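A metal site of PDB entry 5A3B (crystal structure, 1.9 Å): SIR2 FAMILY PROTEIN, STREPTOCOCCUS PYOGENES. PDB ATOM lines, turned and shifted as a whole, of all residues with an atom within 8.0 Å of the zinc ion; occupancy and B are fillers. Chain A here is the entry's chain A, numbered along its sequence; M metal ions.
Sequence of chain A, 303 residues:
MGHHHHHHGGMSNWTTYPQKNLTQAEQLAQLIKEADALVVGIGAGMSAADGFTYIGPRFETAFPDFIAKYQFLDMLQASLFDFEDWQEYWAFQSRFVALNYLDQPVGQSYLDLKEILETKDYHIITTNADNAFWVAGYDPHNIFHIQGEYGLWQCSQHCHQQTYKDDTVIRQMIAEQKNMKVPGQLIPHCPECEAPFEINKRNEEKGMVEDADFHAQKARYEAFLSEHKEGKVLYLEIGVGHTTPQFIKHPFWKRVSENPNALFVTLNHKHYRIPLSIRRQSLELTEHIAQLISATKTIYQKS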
ATOM      1  N   GLN A 154      12.139 -17.726 -25.055  1.00  0.00           N
ATOM      2  CA  GLN A 154      13.388 -17.046 -25.415  1.00  0.00           C
ATOM      3  C   GLN A 154      14.480 -18.079 -25.696  1.00  0.00           C
ATOM      4  O   GLN A 154      14.440 -19.195 -25.212  1.00  0.00           O
ATOM      5  CB  GLN A 154      13.849 -16.085 -24.317  1.00  0.00           C
ATOM      6  CG  GLN A 154      14.346 -16.771 -23.039  1.00  0.00           C
ATOM      7  CD  GLN A 154      14.584 -15.819 -21.861  1.00  0.00           C
ATOM      8  OE1 GLN A 154      14.213 -14.630 -21.887  1.00  0.00           O
ATOM      9  NE2 GLN A 154      15.146 -16.369 -20.792  1.00  0.00           N
ATOM     10  N   CYS A 155      15.477 -17.677 -26.483  1.00  0.00           N
ATOM     11  CA  CYS A 155      16.603 -18.570 -26.748  1.00  0.00           C
ATOM     12  C   CYS A 155      17.337 -18.871 -25.446  1.00  0.00           C
ATOM     13  O   CYS A 155      17.709 -17.970 -24.731  1.00  0.00           O
ATOM     14  CB  CYS A 155      17.580 -17.943 -27.764  1.00  0.00           C
ATOM     15  SG  CYS A 155      19.131 -18.850 -27.819  1.00  0.00           S
ATOM     16  N   SER A 156      17.552 -20.150 -25.123  1.00  0.00           N
ATOM     17  CA  SER A 156      18.210 -20.471 -23.841  1.00  0.00           C
ATOM     18  C   SER A 156      19.625 -19.904 -23.744  1.00  0.00           C
ATOM     19  O   SER A 156      20.159 -19.795 -22.640  1.00  0.00           O
ATOM     20  CB  SER A 156      18.238 -21.982 -23.533  1.00  0.00           C
ATOM     21  OG  SER A 156      18.962 -22.690 -24.519  1.00  0.00           O
ATOM     22  N   GLN A 157      20.224 -19.528 -24.873  1.00  0.00           N
ATOM     23  CA  GLN A 157      21.510 -18.867 -24.880  1.00  0.00           C
ATOM     24  C   GLN A 157      21.369 -17.362 -25.053  1.00  0.00           C
ATOM     25  O   GLN A 157      22.366 -16.660 -25.223  1.00  0.00           O
ATOM     26  CB  GLN A 157      22.370 -19.456 -25.979  1.00  0.00           C
ATOM     27  CG  GLN A 157      22.556 -20.955 -25.831  1.00  0.00           C
ATOM     28  CD  GLN A 157      23.809 -21.316 -25.093  1.00  0.00           C
ATOM     29  OE1 GLN A 157      24.910 -21.115 -25.602  1.00  0.00           O
ATOM     30  NE2 GLN A 157      23.662 -21.866 -23.886  1.00  0.00           N
ATOM     31  N   HIS A 158      20.148 -16.855 -24.965  1.00  0.00           N
ATOM     32  CA  HIS A 158      19.892 -15.426 -25.097  1.00  0.00           C
ATOM     33  C   HIS A 158      20.669 -14.929 -26.299  1.00  0.00           C
ATOM     34  O   HIS A 158      21.314 -13.900 -26.197  1.00  0.00           O
ATOM     35  CB  HIS A 158      20.391 -14.655 -23.847  1.00  0.00           C
ATOM     36  CG  HIS A 158      19.679 -14.961 -22.568  1.00  0.00           C
ATOM     37  ND1 HIS A 158      19.341 -16.239 -22.175  1.00  0.00           N
ATOM     38  CD2 HIS A 158      19.305 -14.150 -21.549  1.00  0.00           C
ATOM     39  CE1 HIS A 158      18.770 -16.198 -20.990  1.00  0.00           C
ATOM     40  NE2 HIS A 158      18.722 -14.939 -20.587  1.00  0.00           N
ATOM     41  N   CYS A 159      20.643 -15.639 -27.429  1.00  0.00           N
ATOM     42  CA  CYS A 159      21.546 -15.289 -28.535  1.00  0.00           C
ATOM     43  C   CYS A 159      21.090 -14.029 -29.314  1.00  0.00           C
ATOM     44  O   CYS A 159      21.928 -13.338 -29.884  1.00  0.00           O
ATOM     45  CB  CYS A 159      21.782 -16.463 -29.478  1.00  0.00           C
ATOM     46  SG  CYS A 159      20.521 -16.760 -30.724  1.00  0.00           S
ATOM     47  N   HIS A 160      19.792 -13.740 -29.296  1.00  0.00           N
ATOM     48  CA  HIS A 160      19.234 -12.509 -29.851  1.00  0.00           C
ATOM     49  C   HIS A 160      17.959 -12.080 -29.088  1.00  0.00           C
ATOM     50  O   HIS A 160      17.268 -12.913 -28.492  1.00  0.00           O
ATOM     51  CB  HIS A 160      18.922 -12.673 -31.345  1.00  0.00           C
ATOM     52  CG  HIS A 160      17.817 -13.647 -31.634  1.00  0.00           C
ATOM     53  ND1 HIS A 160      17.859 -14.970 -31.248  1.00  0.00           N
ATOM     54  CD2 HIS A 160      16.648 -13.494 -32.301  1.00  0.00           C
ATOM     55  CE1 HIS A 160      16.761 -15.586 -31.663  1.00  0.00           C
ATOM     56  NE2 HIS A 160      16.006 -14.713 -32.296  1.00  0.00           N
ATOM     57  N   TYR A 164       9.292 -15.554 -28.620  1.00  0.00           N
ATOM     58  CA  TYR A 164       8.480 -16.370 -29.519  1.00  0.00           C
ATOM     59  C   TYR A 164       7.363 -16.995 -28.725  1.00  0.00           C
ATOM     60  O   TYR A 164       7.452 -17.123 -27.513  1.00  0.00           O
ATOM     61  CB  TYR A 164       9.319 -17.504 -30.090  1.00  0.00           C
ATOM     62  CG  TYR A 164      10.467 -17.019 -30.919  1.00  0.00           C
ATOM     63  CD1 TYR A 164      11.601 -16.496 -30.316  1.00  0.00           C
ATOM     64  CD2 TYR A 164      10.428 -17.075 -32.309  1.00  0.00           C
ATOM     65  CE1 TYR A 164      12.650 -16.052 -31.054  1.00  0.00           C
ATOM     66  CE2 TYR A 164      11.505 -16.628 -33.059  1.00  0.00           C
ATOM     67  CZ  TYR A 164      12.607 -16.130 -32.408  1.00  0.00           C
ATOM     68  OH  TYR A 164      13.685 -15.650 -33.079  1.00  0.00           O
ATOM     69  N   HIS A 189      13.489 -25.280 -30.756  1.00  0.00           N
ATOM     70  CA  HIS A 189      14.863 -24.726 -30.830  1.00  0.00           C
ATOM     71  C   HIS A 189      14.874 -23.363 -31.480  1.00  0.00           C
ATOM     72  O   HIS A 189      14.106 -23.083 -32.404  1.00  0.00           O
ATOM     73  CB  HIS A 189      15.789 -25.641 -31.633  1.00  0.00           C
ATOM     74  CG  HIS A 189      16.077 -26.941 -30.947  1.00  0.00           C
ATOM     75  ND1 HIS A 189      15.332 -28.078 -31.168  1.00  0.00           N
ATOM     76  CD2 HIS A 189      17.008 -27.276 -30.023  1.00  0.00           C
ATOM     77  CE1 HIS A 189      15.789 -29.052 -30.402  1.00  0.00           C
ATOM     78  NE2 HIS A 189      16.798 -28.593 -29.701  1.00  0.00           N
ATOM     79  N   CYS A 190      15.746 -22.501 -30.966  1.00  0.00           N
ATOM     80  CA  CYS A 190      15.996 -21.177 -31.515  1.00  0.00           C
ATOM     81  C   CYS A 190      16.436 -21.320 -32.971  1.00  0.00           C
ATOM     82  O   CYS A 190      17.381 -22.060 -33.250  1.00  0.00           O
ATOM     83  CB  CYS A 190      17.059 -20.477 -30.681  1.00  0.00           C
ATOM     84  SG  CYS A 190      17.822 -18.976 -31.378  1.00  0.00           S
ATOM     85  N   PRO A 191      15.747 -20.652 -33.903  1.00  0.00           N
ATOM     86  CA  PRO A 191      16.175 -20.745 -35.302  1.00  0.00           C
ATOM     87  C   PRO A 191      17.538 -20.113 -35.622  1.00  0.00           C
ATOM     88  O   PRO A 191      18.114 -20.493 -36.642  1.00  0.00           O
ATOM     89  CB  PRO A 191      15.071 -20.000 -36.060  1.00  0.00           C
ATOM     90  CG  PRO A 191      14.390 -19.140 -35.041  1.00  0.00           C
ATOM     91  CD  PRO A 191      14.524 -19.850 -33.730  1.00  0.00           C
ATOM     92  N   GLU A 192      18.036 -19.201 -34.795  1.00  0.00           N
ATOM     93  CA  GLU A 192      19.330 -18.561 -35.033  1.00  0.00           C
ATOM     94  C   GLU A 192      20.511 -19.441 -34.647  1.00  0.00           C
ATOM     95  O   GLU A 192      21.491 -19.523 -35.372  1.00  0.00           O
ATOM     96  CB  GLU A 192      19.469 -17.253 -34.261  1.00  0.00           C
ATOM     97  CG  GLU A 192      18.443 -16.195 -34.596  1.00  0.00           C
ATOM     98  CD  GLU A 192      18.494 -15.800 -36.036  1.00  0.00           C
ATOM     99  OE1 GLU A 192      19.600 -15.491 -36.527  1.00  0.00           O
ATOM    100  OE2 GLU A 192      17.424 -15.814 -36.698  1.00  0.00           O
ATOM    101  N   CYS A 193      20.450 -20.067 -33.479  1.00  0.00           N
ATOM    102  CA  CYS A 193      21.602 -20.765 -32.956  1.00  0.00           C
ATOM    103  C   CYS A 193      21.355 -22.247 -32.648  1.00  0.00           C
ATOM    104  O   CYS A 193      22.249 -22.934 -32.194  1.00  0.00           O
ATOM    105  CB  CYS A 193      22.106 -20.009 -31.723  1.00  0.00           C
ATOM    106  SG  CYS A 193      21.162 -20.306 -30.202  1.00  0.00           S
ATOM    107  N   GLU A 194      20.121 -22.716 -32.875  1.00  0.00           N
ATOM    108  CA  GLU A 194      19.671 -24.090 -32.562  1.00  0.00           C
ATOM    109  C   GLU A 194      19.719 -24.538 -31.086  1.00  0.00           C
ATOM    110  O   GLU A 194      19.438 -25.694 -30.786  1.00  0.00           O
ATOM    111  CB  GLU A 194      20.361 -25.101 -33.499  1.00  0.00           C
ATOM    112  CG  GLU A 194      19.790 -25.039 -34.910  1.00  0.00           C
ATOM    113  CD  GLU A 194      18.330 -25.501 -34.971  1.00  0.00           C
ATOM    114  OE1 GLU A 194      18.108 -26.742 -34.929  1.00  0.00           O
ATOM    115  OE2 GLU A 194      17.396 -24.633 -35.022  1.00  0.00           O
ATOM    116  N   ALA A 195      20.022 -23.639 -30.162  1.00  0.00           N
ATOM    117  CA  ALA A 195      19.868 -23.967 -28.756  1.00  0.00           C
ATOM    118  C   ALA A 195      18.361 -24.208 -28.456  1.00  0.00           C
ATOM    119  O   ALA A 195      17.490 -23.655 -29.101  1.00  0.00           O
ATOM    120  CB  ALA A 195      20.418 -22.855 -27.899  1.00  0.00           C
ATOM    121  N   PRO A 196      18.062 -25.021 -27.430  1.00  0.00           N
ATOM    122  CA  PRO A 196      16.636 -25.135 -27.126  1.00  0.00           C
ATOM    123  C   PRO A 196      16.035 -23.794 -26.685  1.00  0.00           C
ATOM    124  O   PRO A 196      16.747 -22.942 -26.126  1.00  0.00           O
ATOM    125  CB  PRO A 196      16.586 -26.164 -25.993  1.00  0.00           C
ATOM    126  CG  PRO A 196      17.903 -26.891 -26.050  1.00  0.00           C
ATOM    127  CD  PRO A 196      18.900 -25.887 -26.591  1.00  0.00           C
ATOM    128  N   PHE A 197      14.741 -23.611 -26.968  1.00  0.00           N
ATOM    129  CA  PHE A 197      13.970 -22.542 -26.355  1.00  0.00           C
ATOM    130  C   PHE A 197      13.755 -22.890 -24.901  1.00  0.00           C
ATOM    131  O   PHE A 197      13.794 -24.079 -24.497  1.00  0.00           O
ATOM    132  CB  PHE A 197      12.607 -22.345 -27.031  1.00  0.00           C
ATOM    133  CG  PHE A 197      12.626 -21.442 -28.221  1.00  0.00           C
ATOM    134  CD1 PHE A 197      13.222 -20.206 -28.163  1.00  0.00           C
ATOM    135  CD2 PHE A 197      12.040 -21.828 -29.422  1.00  0.00           C
ATOM    136  CE1 PHE A 197      13.234 -19.347 -29.247  1.00  0.00           C
ATOM    137  CE2 PHE A 197      12.043 -20.980 -30.523  1.00  0.00           C
ATOM    138  CZ  PHE A 197      12.656 -19.730 -30.436  1.00  0.00           C
HETATM  139 ZN    ZN M   1      19.578 -18.720 -30.142  1.00  0.00          ZN
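SG of Cys 159 sits close to ND1 of His 160.
The backbone carbonyl oxygen of Cys 155 lies close to a ring nitrogen (ND1) of His 158, 3.5 Å away.
SG of Cys 190 lies close to N of Glu 192 (3.4 Å).
The side-chain sulfur (SG) of Cys 193 lies close to the backbone NH (N) of Ala 195 (3.5 Å).
N of Gln 157 lies close to SG of Cys 155.
The backbone carbonyl oxygen (O) of Ala 195 sits at hydrogen-bond distance from the backbone NH (N) of Cys 190, at 2.8 Å.
Four residues have an atom within 4 Å of the zinc ion: Cys 155, Cys 159, Cys 190 and Cys 193.
Along chain A the residues within 4 Å of the zinc ion span positions 155 to 193.
The nearest printed residue that does not touch the zinc ion is His 160 (4.3 Å).
The zinc ion is bound by the side-chain sulfur (SG) of Cys 190, the side-chain sulfur (SG) of Cys 193, the side-chain sulfur (SG) of Cys 159 and the side-chain sulfur (SG) of Cys 155.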
